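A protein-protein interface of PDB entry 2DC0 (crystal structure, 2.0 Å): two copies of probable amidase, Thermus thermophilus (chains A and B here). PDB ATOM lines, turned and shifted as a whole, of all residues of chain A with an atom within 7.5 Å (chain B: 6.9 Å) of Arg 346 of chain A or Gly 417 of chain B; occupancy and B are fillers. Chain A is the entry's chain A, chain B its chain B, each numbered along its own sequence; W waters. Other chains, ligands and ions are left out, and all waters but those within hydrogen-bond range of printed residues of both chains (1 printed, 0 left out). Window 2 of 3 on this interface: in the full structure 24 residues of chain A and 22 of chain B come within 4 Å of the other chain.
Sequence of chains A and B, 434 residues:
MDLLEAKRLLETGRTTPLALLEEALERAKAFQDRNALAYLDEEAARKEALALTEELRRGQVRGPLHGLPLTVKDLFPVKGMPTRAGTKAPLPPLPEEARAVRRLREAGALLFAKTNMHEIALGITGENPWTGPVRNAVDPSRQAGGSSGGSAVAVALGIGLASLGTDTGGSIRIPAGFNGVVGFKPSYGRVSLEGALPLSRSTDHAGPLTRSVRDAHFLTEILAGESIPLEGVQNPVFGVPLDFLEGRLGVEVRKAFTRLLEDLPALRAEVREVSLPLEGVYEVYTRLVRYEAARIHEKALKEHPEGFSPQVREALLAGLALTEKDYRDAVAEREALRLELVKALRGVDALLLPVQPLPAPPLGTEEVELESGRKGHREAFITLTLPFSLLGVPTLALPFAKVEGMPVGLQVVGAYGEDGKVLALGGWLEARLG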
ATOM      1  N   ARG A 272      -8.962  25.212  -2.060  1.00  0.00           N
ATOM      2  CA  ARG A 272      -7.992  26.234  -2.432  1.00  0.00           C
ATOM      3  C   ARG A 272      -7.977  26.442  -3.936  1.00  0.00           C
ATOM      4  O   ARG A 272      -7.991  25.481  -4.705  1.00  0.00           O
ATOM      5  CB  ARG A 272      -6.581  25.837  -1.983  1.00  0.00           C
ATOM      6  CG  ARG A 272      -6.409  25.653  -0.478  1.00  0.00           C
ATOM      7  CD  ARG A 272      -4.968  25.249  -0.139  1.00  0.00           C
ATOM      8  NE  ARG A 272      -4.815  24.890   1.271  1.00  0.00           N
ATOM      9  CZ  ARG A 272      -3.685  24.451   1.819  1.00  0.00           C
ATOM     10  NH1 ARG A 272      -2.593  24.313   1.077  1.00  0.00           N
ATOM     11  NH2 ARG A 272      -3.650  24.144   3.112  1.00  0.00           N
ATOM     12  N   VAL A 274      -6.321  27.145  -7.414  1.00  0.00           N
ATOM     13  CA  VAL A 274      -5.000  26.857  -7.967  1.00  0.00           C
ATOM     14  C   VAL A 274      -5.004  27.363  -9.401  1.00  0.00           C
ATOM     15  O   VAL A 274      -6.070  27.559  -9.988  1.00  0.00           O
ATOM     16  CB  VAL A 274      -4.667  25.332  -7.991  1.00  0.00           C
ATOM     17  CG1 VAL A 274      -4.647  24.768  -6.577  1.00  0.00           C
ATOM     18  CG2 VAL A 274      -5.669  24.591  -8.861  1.00  0.00           C
ATOM     19  N   ARG A 338       3.510  19.785 -18.697  1.00  0.00           N
ATOM     20  CA  ARG A 338       3.665  18.902 -17.551  1.00  0.00           C
ATOM     21  C   ARG A 338       3.983  19.628 -16.243  1.00  0.00           C
ATOM     22  O   ARG A 338       3.367  19.342 -15.217  1.00  0.00           O
ATOM     23  CB  ARG A 338       4.734  17.841 -17.866  1.00  0.00           C
ATOM     24  CG  ARG A 338       4.625  16.580 -17.022  1.00  0.00           C
ATOM     25  CD  ARG A 338       5.565  15.479 -17.521  1.00  0.00           C
ATOM     26  NE  ARG A 338       5.289  15.068 -18.898  1.00  0.00           N
ATOM     27  CZ  ARG A 338       4.306  14.248 -19.267  1.00  0.00           C
ATOM     28  NH1 ARG A 338       3.482  13.732 -18.364  1.00  0.00           N
ATOM     29  NH2 ARG A 338       4.153  13.933 -20.548  1.00  0.00           N
ATOM     30  N   LEU A 339       4.918  20.577 -16.270  1.00  0.00           N
ATOM     31  CA  LEU A 339       5.275  21.298 -15.042  1.00  0.00           C
ATOM     32  C   LEU A 339       4.089  22.080 -14.463  1.00  0.00           C
ATOM     33  O   LEU A 339       3.951  22.198 -13.241  1.00  0.00           O
ATOM     34  CB  LEU A 339       6.461  22.246 -15.291  1.00  0.00           C
ATOM     35  CG  LEU A 339       7.014  23.015 -14.085  1.00  0.00           C
ATOM     36  CD1 LEU A 339       7.428  22.044 -12.978  1.00  0.00           C
ATOM     37  CD2 LEU A 339       8.208  23.863 -14.523  1.00  0.00           C
ATOM     38  N   GLU A 340       3.233  22.605 -15.339  1.00  0.00           N
ATOM     39  CA  GLU A 340       2.050  23.361 -14.912  1.00  0.00           C
ATOM     40  C   GLU A 340       1.098  22.522 -14.066  1.00  0.00           C
ATOM     41  O   GLU A 340       0.553  22.995 -13.064  1.00  0.00           O
ATOM     42  CB  GLU A 340       1.269  23.882 -16.120  1.00  0.00           C
ATOM     43  CG  GLU A 340       1.776  25.179 -16.697  1.00  0.00           C
ATOM     44  CD  GLU A 340       0.849  25.720 -17.765  1.00  0.00           C
ATOM     45  OE1 GLU A 340      -0.381  25.719 -17.539  1.00  0.00           O
ATOM     46  OE2 GLU A 340       1.353  26.148 -18.824  1.00  0.00           O
ATOM     47  N   LEU A 341       0.872  21.287 -14.491  1.00  0.00           N
ATOM     48  CA  LEU A 341      -0.013  20.400 -13.753  1.00  0.00           C
ATOM     49  C   LEU A 341       0.624  20.017 -12.414  1.00  0.00           C
ATOM     50  O   LEU A 341      -0.051  19.978 -11.385  1.00  0.00           O
ATOM     51  CB  LEU A 341      -0.315  19.140 -14.571  1.00  0.00           C
ATOM     52  CG  LEU A 341      -1.201  18.101 -13.864  1.00  0.00           C
ATOM     53  CD1 LEU A 341      -2.469  18.771 -13.337  1.00  0.00           C
ATOM     54  CD2 LEU A 341      -1.552  16.976 -14.835  1.00  0.00           C
ATOM     55  N   VAL A 342       1.925  19.743 -12.434  1.00  0.00           N
ATOM     56  CA  VAL A 342       2.652  19.379 -11.225  1.00  0.00           C
ATOM     57  C   VAL A 342       2.544  20.492 -10.184  1.00  0.00           C
ATOM     58  O   VAL A 342       2.329  20.235  -8.992  1.00  0.00           O
ATOM     59  CB  VAL A 342       4.144  19.109 -11.545  1.00  0.00           C
ATOM     60  CG1 VAL A 342       4.948  18.946 -10.257  1.00  0.00           C
ATOM     61  CG2 VAL A 342       4.262  17.848 -12.399  1.00  0.00           C
ATOM     62  N   LYS A 343       2.686  21.731 -10.641  1.00  0.00           N
ATOM     63  CA  LYS A 343       2.603  22.890  -9.759  1.00  0.00           C
ATOM     64  C   LYS A 343       1.195  23.083  -9.197  1.00  0.00           C
ATOM     65  O   LYS A 343       1.031  23.452  -8.033  1.00  0.00           O
ATOM     66  CB  LYS A 343       3.055  24.149 -10.513  1.00  0.00           C
ATOM     67  CG  LYS A 343       4.536  24.125 -10.866  1.00  0.00           C
ATOM     68  CD  LYS A 343       4.934  25.206 -11.862  1.00  0.00           C
ATOM     69  CE  LYS A 343       4.958  26.592 -11.252  1.00  0.00           C
ATOM     70  NZ  LYS A 343       5.525  27.566 -12.231  1.00  0.00           N
ATOM     71  N   ALA A 344       0.180  22.823 -10.010  1.00  0.00           N
ATOM     72  CA  ALA A 344      -1.190  22.987  -9.542  1.00  0.00           C
ATOM     73  C   ALA A 344      -1.528  21.964  -8.458  1.00  0.00           C
ATOM     74  O   ALA A 344      -2.307  22.252  -7.556  1.00  0.00           O
ATOM     75  CB  ALA A 344      -2.169  22.858 -10.713  1.00  0.00           C
ATOM     76  N   LEU A 345      -0.936  20.775  -8.551  1.00  0.00           N
ATOM     77  CA  LEU A 345      -1.189  19.710  -7.584  1.00  0.00           C
ATOM     78  C   LEU A 345      -0.385  19.838  -6.293  1.00  0.00           C
ATOM     79  O   LEU A 345      -0.758  19.267  -5.268  1.00  0.00           O
ATOM     80  CB  LEU A 345      -0.909  18.342  -8.219  1.00  0.00           C
ATOM     81  CG  LEU A 345      -1.964  17.818  -9.196  1.00  0.00           C
ATOM     82  CD1 LEU A 345      -1.433  16.601  -9.935  1.00  0.00           C
ATOM     83  CD2 LEU A 345      -3.238  17.473  -8.428  1.00  0.00           C
ATOM     84  N   ARG A 346       0.718  20.580  -6.340  1.00  0.00           N
ATOM     85  CA  ARG A 346       1.557  20.759  -5.156  1.00  0.00           C
ATOM     86  C   ARG A 346       0.792  21.417  -4.012  1.00  0.00           C
ATOM     87  O   ARG A 346       0.184  22.469  -4.188  1.00  0.00           O
ATOM     88  CB  ARG A 346       2.786  21.614  -5.489  1.00  0.00           C
ATOM     89  CG  ARG A 346       3.855  20.904  -6.300  1.00  0.00           C
ATOM     90  CD  ARG A 346       5.019  21.843  -6.617  1.00  0.00           C
ATOM     91  NE  ARG A 346       5.662  22.368  -5.411  1.00  0.00           N
ATOM     92  CZ  ARG A 346       6.458  21.664  -4.611  1.00  0.00           C
ATOM     93  NH1 ARG A 346       6.724  20.392  -4.882  1.00  0.00           N
ATOM     94  NH2 ARG A 346       6.984  22.230  -3.530  1.00  0.00           N
ATOM     95  N   GLY A 347       0.818  20.797  -2.840  1.00  0.00           N
ATOM     96  CA  GLY A 347       0.130  21.384  -1.703  1.00  0.00           C
ATOM     97  C   GLY A 347      -1.334  21.015  -1.532  1.00  0.00           C
ATOM     98  O   GLY A 347      -1.936  21.394  -0.532  1.00  0.00           O
ATOM     99  N   VAL A 348      -1.919  20.307  -2.497  1.00  0.00           N
ATOM    100  CA  VAL A 348      -3.318  19.884  -2.388  1.00  0.00           C
ATOM    101  C   VAL A 348      -3.387  18.369  -2.571  1.00  0.00           C
ATOM    102  O   VAL A 348      -2.475  17.764  -3.135  1.00  0.00           O
ATOM    103  CB  VAL A 348      -4.247  20.579  -3.444  1.00  0.00           C
ATOM    104  CG1 VAL A 348      -4.224  22.091  -3.250  1.00  0.00           C
ATOM    105  CG2 VAL A 348      -3.822  20.222  -4.864  1.00  0.00           C
ATOM    106  N   ASP A 349      -4.456  17.746  -2.085  1.00  0.00           N
ATOM    107  CA  ASP A 349      -4.582  16.297  -2.214  1.00  0.00           C
ATOM    108  C   ASP A 349      -5.051  15.904  -3.609  1.00  0.00           C
ATOM    109  O   ASP A 349      -4.710  14.833  -4.115  1.00  0.00           O
ATOM    110  CB  ASP A 349      -5.532  15.752  -1.146  1.00  0.00           C
ATOM    111  CG  ASP A 349      -4.981  15.935   0.260  1.00  0.00           C
ATOM    112  OD1 ASP A 349      -3.819  15.537   0.486  1.00  0.00           O
ATOM    113  OD2 ASP A 349      -5.700  16.472   1.130  1.00  0.00           O
ATOM    114  N   LEU A 351      -7.239  17.755  -7.427  1.00  0.00           N
ATOM    115  CA  LEU A 351      -7.928  18.857  -8.064  1.00  0.00           C
ATOM    116  C   LEU A 351      -9.357  18.376  -8.245  1.00  0.00           C
ATOM    117  O   LEU A 351      -9.601  17.177  -8.391  1.00  0.00           O
ATOM    118  CB  LEU A 351      -7.332  19.169  -9.442  1.00  0.00           C
ATOM    119  CG  LEU A 351      -5.842  19.502  -9.504  1.00  0.00           C
ATOM    120  CD1 LEU A 351      -5.481  19.961 -10.911  1.00  0.00           C
ATOM    121  CD2 LEU A 351      -5.518  20.581  -8.485  1.00  0.00           C
ATOM    122  N   ALA A 415      -1.960  13.240  -8.433  1.00  0.00           N
ATOM    123  CA  ALA A 415      -0.613  13.249  -8.988  1.00  0.00           C
ATOM    124  C   ALA A 415      -0.344  11.911  -9.662  1.00  0.00           C
ATOM    125  O   ALA A 415      -0.989  10.913  -9.355  1.00  0.00           O
ATOM    126  CB  ALA A 415       0.421  13.489  -7.875  1.00  0.00           C
ATOM    127  N   SER B 187      13.575  21.073 -13.497  1.00  0.00           N
ATOM    128  CA  SER B 187      12.514  20.268 -14.073  1.00  0.00           C
ATOM    129  C   SER B 187      12.383  20.795 -15.498  1.00  0.00           C
ATOM    130  O   SER B 187      12.618  21.978 -15.746  1.00  0.00           O
ATOM    131  CB  SER B 187      11.191  20.487 -13.329  1.00  0.00           C
ATOM    132  OG  SER B 187      11.278  20.108 -11.973  1.00  0.00           O
ATOM    133  N   TYR B 188      12.014  19.930 -16.434  1.00  0.00           N
ATOM    134  CA  TYR B 188      11.861  20.360 -17.819  1.00  0.00           C
ATOM    135  C   TYR B 188      10.900  21.551 -17.914  1.00  0.00           C
ATOM    136  O   TYR B 188       9.891  21.599 -17.214  1.00  0.00           O
ATOM    137  CB  TYR B 188      11.329  19.210 -18.676  1.00  0.00           C
ATOM    138  CG  TYR B 188      11.070  19.588 -20.122  1.00  0.00           C
ATOM    139  CD1 TYR B 188      12.070  19.470 -21.089  1.00  0.00           C
ATOM    140  CD2 TYR B 188       9.818  20.068 -20.521  1.00  0.00           C
ATOM    141  CE1 TYR B 188      11.827  19.815 -22.422  1.00  0.00           C
ATOM    142  CE2 TYR B 188       9.566  20.419 -21.846  1.00  0.00           C
ATOM    143  CZ  TYR B 188      10.572  20.288 -22.790  1.00  0.00           C
ATOM    144  OH  TYR B 188      10.315  20.611 -24.101  1.00  0.00           O
ATOM    145  N   ARG B 190      11.185  24.485 -16.807  1.00  0.00           N
ATOM    146  CA  ARG B 190      11.341  25.476 -15.745  1.00  0.00           C
ATOM    147  C   ARG B 190      12.015  26.737 -16.302  1.00  0.00           C
ATOM    148  O   ARG B 190      11.521  27.851 -16.128  1.00  0.00           O
ATOM    149  CB  ARG B 190      12.167  24.881 -14.596  1.00  0.00           C
ATOM    150  CG  ARG B 190      12.515  25.855 -13.476  1.00  0.00           C
ATOM    151  CD  ARG B 190      11.345  26.113 -12.543  1.00  0.00           C
ATOM    152  NE  ARG B 190      11.016  24.951 -11.717  1.00  0.00           N
ATOM    153  CZ  ARG B 190      10.039  24.940 -10.813  1.00  0.00           C
ATOM    154  NH1 ARG B 190       9.301  26.023 -10.625  1.00  0.00           N
ATOM    155  NH2 ARG B 190       9.792  23.853 -10.097  1.00  0.00           N
ATOM    156  N   ILE B 228      11.853  29.981  -5.984  1.00  0.00           N
ATOM    157  CA  ILE B 228      11.816  28.548  -5.743  1.00  0.00           C
ATOM    158  C   ILE B 228      12.158  28.332  -4.274  1.00  0.00           C
ATOM    159  O   ILE B 228      13.309  28.122  -3.922  1.00  0.00           O
ATOM    160  CB  ILE B 228      12.850  27.834  -6.627  1.00  0.00           C
ATOM    161  CG1 ILE B 228      12.553  28.141  -8.101  1.00  0.00           C
ATOM    162  CG2 ILE B 228      12.831  26.340  -6.363  1.00  0.00           C
ATOM    163  CD1 ILE B 228      13.679  27.791  -9.072  1.00  0.00           C
ATOM    164  N   PRO B 229      11.155  28.398  -3.394  1.00  0.00           N
ATOM    165  CA  PRO B 229      11.342  28.213  -1.952  1.00  0.00           C
ATOM    166  C   PRO B 229      12.200  27.011  -1.559  1.00  0.00           C
ATOM    167  O   PRO B 229      12.093  25.934  -2.145  1.00  0.00           O
ATOM    168  CB  PRO B 229       9.911  28.093  -1.439  1.00  0.00           C
ATOM    169  CG  PRO B 229       9.171  29.027  -2.340  1.00  0.00           C
ATOM    170  CD  PRO B 229       9.739  28.661  -3.704  1.00  0.00           C
ATOM    171  N   GLU B 231      13.205  24.490   1.565  1.00  0.00           N
ATOM    172  CA  GLU B 231      12.687  24.048   2.852  1.00  0.00           C
ATOM    173  C   GLU B 231      13.809  23.501   3.722  1.00  0.00           C
ATOM    174  O   GLU B 231      14.925  23.284   3.250  1.00  0.00           O
ATOM    175  CB  GLU B 231      11.609  22.983   2.648  1.00  0.00           C
ATOM    176  CG  GLU B 231      10.383  23.494   1.894  1.00  0.00           C
ATOM    177  CD  GLU B 231       9.604  24.536   2.680  1.00  0.00           C
ATOM    178  OE1 GLU B 231       9.011  24.175   3.722  1.00  0.00           O
ATOM    179  OE2 GLU B 231       9.589  25.716   2.261  1.00  0.00           O
ATOM    180  N   GLY B 392      12.523  14.366 -17.562  1.00  0.00           N
ATOM    181  CA  GLY B 392      12.384  15.740 -17.100  1.00  0.00           C
ATOM    182  C   GLY B 392      12.421  16.102 -15.624  1.00  0.00           C
ATOM    183  O   GLY B 392      12.062  17.221 -15.274  1.00  0.00           O
ATOM    184  N   VAL B 393      12.866  15.201 -14.758  1.00  0.00           N
ATOM    185  CA  VAL B 393      12.894  15.500 -13.328  1.00  0.00           C
ATOM    186  C   VAL B 393      14.110  16.326 -12.894  1.00  0.00           C
ATOM    187  O   VAL B 393      15.209  16.158 -13.426  1.00  0.00           O
ATOM    188  CB  VAL B 393      12.820  14.193 -12.511  1.00  0.00           C
ATOM    189  CG1 VAL B 393      11.441  13.562 -12.691  1.00  0.00           C
ATOM    190  CG2 VAL B 393      13.894  13.213 -12.982  1.00  0.00           C
ATOM    191  N   PRO B 394      13.925  17.234 -11.913  1.00  0.00           N
ATOM    192  CA  PRO B 394      15.034  18.071 -11.436  1.00  0.00           C
ATOM    193  C   PRO B 394      16.183  17.226 -10.910  1.00  0.00           C
ATOM    194  O   PRO B 394      15.985  16.348 -10.078  1.00  0.00           O
ATOM    195  CB  PRO B 394      14.378  18.943 -10.363  1.00  0.00           C
ATOM    196  CG  PRO B 394      13.257  18.084  -9.848  1.00  0.00           C
ATOM    197  CD  PRO B 394      12.708  17.459 -11.110  1.00  0.00           C
ATOM    198  N   GLY B 414      15.105  14.403  -7.855  1.00  0.00           N
ATOM    199  CA  GLY B 414      13.847  14.598  -7.155  1.00  0.00           C
ATOM    200  C   GLY B 414      12.677  14.422  -8.103  1.00  0.00           C
ATOM    201  O   GLY B 414      12.865  14.308  -9.317  1.00  0.00           O
ATOM    202  N   ALA B 415      11.468  14.395  -7.555  1.00  0.00           N
ATOM    203  CA  ALA B 415      10.274  14.245  -8.373  1.00  0.00           C
ATOM    204  C   ALA B 415      10.076  15.503  -9.209  1.00  0.00           C
ATOM    205  O   ALA B 415      10.591  16.577  -8.874  1.00  0.00           O
ATOM    206  CB  ALA B 415       9.049  14.007  -7.486  1.00  0.00           C
ATOM    207  N   TYR B 416       9.326  15.365 -10.296  1.00  0.00           N
ATOM    208  CA  TYR B 416       9.039  16.486 -11.194  1.00  0.00           C
ATOM    209  C   TYR B 416       8.527  17.664 -10.366  1.00  0.00           C
ATOM    210  O   TYR B 416       7.632  17.497  -9.539  1.00  0.00           O
ATOM    211  CB  TYR B 416       7.957  16.075 -12.197  1.00  0.00           C
ATOM    212  CG  TYR B 416       8.102  16.671 -13.583  1.00  0.00           C
ATOM    213  CD1 TYR B 416       8.542  15.889 -14.649  1.00  0.00           C
ATOM    214  CD2 TYR B 416       7.769  18.006 -13.835  1.00  0.00           C
ATOM    215  CE1 TYR B 416       8.641  16.409 -15.936  1.00  0.00           C
ATOM    216  CE2 TYR B 416       7.871  18.541 -15.120  1.00  0.00           C
ATOM    217  CZ  TYR B 416       8.306  17.731 -16.167  1.00  0.00           C
ATOM    218  OH  TYR B 416       8.391  18.240 -17.449  1.00  0.00           O
ATOM    219  N   GLY B 417       9.096  18.845 -10.585  1.00  0.00           N
ATOM    220  CA  GLY B 417       8.656  20.022  -9.858  1.00  0.00           C
ATOM    221  C   GLY B 417       9.284  20.272  -8.495  1.00  0.00           C
ATOM    222  O   GLY B 417       9.098  21.346  -7.926  1.00  0.00           O
ATOM    223  N   GLU B 418      10.021  19.299  -7.966  1.00  0.00           N
ATOM    224  CA  GLU B 418      10.666  19.448  -6.658  1.00  0.00           C
ATOM    225  C   GLU B 418      12.041  20.116  -6.729  1.00  0.00           C
ATOM    226  O   GLU B 418      12.948  19.758  -5.974  1.00  0.00           O
ATOM    227  CB  GLU B 418      10.818  18.082  -5.969  1.00  0.00           C
ATOM    228  CG  GLU B 418       9.505  17.392  -5.605  1.00  0.00           C
ATOM    229  CD  GLU B 418       9.705  16.166  -4.717  1.00  0.00           C
ATOM    230  OE1 GLU B 418      10.646  15.374  -4.970  1.00  0.00           O
ATOM    231  OE2 GLU B 418       8.906  15.975  -3.771  1.00  0.00           O
ATOM    232  N   ASP B 419      12.194  21.090  -7.620  1.00  0.00           N
ATOM    233  CA  ASP B 419      13.472  21.788  -7.768  1.00  0.00           C
ATOM    234  C   ASP B 419      14.001  22.320  -6.437  1.00  0.00           C
ATOM    235  O   ASP B 419      15.177  22.161  -6.122  1.00  0.00           O
ATOM    236  CB  ASP B 419      13.330  22.950  -8.755  1.00  0.00           C
ATOM    237  CG  ASP B 419      12.897  22.494 -10.131  1.00  0.00           C
ATOM    238  OD1 ASP B 419      13.656  22.691 -11.094  1.00  0.00           O
ATOM    239  OD2 ASP B 419      11.787  21.939 -10.248  1.00  0.00           O
ATOM    240  N   GLY B 420      13.128  22.958  -5.662  1.00  0.00           N
ATOM    241  CA  GLY B 420      13.539  23.515  -4.382  1.00  0.00           C
ATOM    242  C   GLY B 420      14.037  22.479  -3.387  1.00  0.00           C
ATOM    243  O   GLY B 420      15.014  22.710  -2.671  1.00  0.00           O
ATOM    244  N   LYS B 421      13.362  21.336  -3.336  1.00  0.00           N
ATOM    245  CA  LYS B 421      13.742  20.268  -2.424  1.00  0.00           C
ATOM    246  C   LYS B 421      15.086  19.660  -2.834  1.00  0.00           C
ATOM    247  O   LYS B 421      15.942  19.387  -1.986  1.00  0.00           O
ATOM    248  CB  LYS B 421      12.646  19.194  -2.391  1.00  0.00           C
ATOM    249  CG  LYS B 421      12.912  18.059  -1.412  1.00  0.00           C
ATOM    250  CD  LYS B 421      11.690  17.170  -1.243  1.00  0.00           C
ATOM    251  CE  LYS B 421      11.938  16.112  -0.185  1.00  0.00           C
ATOM    252  NZ  LYS B 421      10.704  15.342   0.145  1.00  0.00           N
HETATM  253  O   HOH W   1       7.075  21.034 -18.090  1.00  0.00           O
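Arg 346 of chain A touches just one residue of chain B: Gly 417 (3.98 Å). Printed residues of chain A within 4 Å of Tyr 188 of chain B: Leu 339 (3.9 Å). Of the printed residues of chain B, Leu 339 of chain A touches Tyr 188, Arg 190, Tyr 416 and Gly 417. Of the printed residues of chain B, Arg 338 of chain A touches Tyr 416 (3.6 Å). The nearest residue of chain B that does not touch Arg 346 of chain A is Glu 418 of chain B (4.2 Å). The nearest printed residue of chain B that does not touch Leu 339 of chain A is Ser 187 of chain B (4.1 Å).
Of the 16 printed residues of chain A, 4 touch a printed residue of chain B. Printed residues of chain B that touch a printed residue of chain A: Tyr 188, Arg 190, Tyr 416 and Gly 417. Along chain B the printed residues that touch a printed residue of chain A span positions 188 to 417. Among the printed residues, no Asp or Glu carboxylate lies within 4 Å of a Lys or Arg side-chain nitrogen of the other chain.
NH2 of Arg 190 of chain B lies within salt-bridge range of OD2 of Asp 419 of chain B, 2.8 Å away. N of Gly 417 of chain B is in hydrogen-bond range of OG of Ser 187 of chain B, at 2.9 Å. The backbone NH of Tyr 188 of chain B lies within hydrogen-bond range of the backbone carbonyl oxygen of Gly 392 of chain B, at 2.9 Å. The backbone carbonyl oxygen of Gly 417 of chain B sits at hydrogen-bond distance from the guanidinium group of Arg 190 of chain B.
1 position is printed for both chains. Of the 8 pairs that touch across the chains among the printed residues, none has its exchanged pair printed and touching as well.
Arg 338 of chain A touches Tyr 416 of chain B. Leu 339 of chain A touches Tyr 188 of chain B. Arg 190 of chain B touches Leu 339 of chain A. CE2 of Tyr 416 of chain B touches N of Leu 339 of chain A (3.8 Å). Gly 417 of chain B touches Leu 339 of chain A. Val 342 of chain A touches Tyr 416 of chain B (CG1 to O, 3.1 Å). Val 342 of chain A touches Gly 417 of chain B. NH1 of Arg 346 of chain A touches O of Gly 417 of chain B (3.98 Å).
Water W1 lies within hydrogen-bond range of the backbone NH of Leu 339 of chain A (2.9 Å), the backbone carbonyl oxygen of Tyr 188 of chain B (3.0 Å) and the side-chain hydroxyl of Tyr 416 of chain B (3.2 Å).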
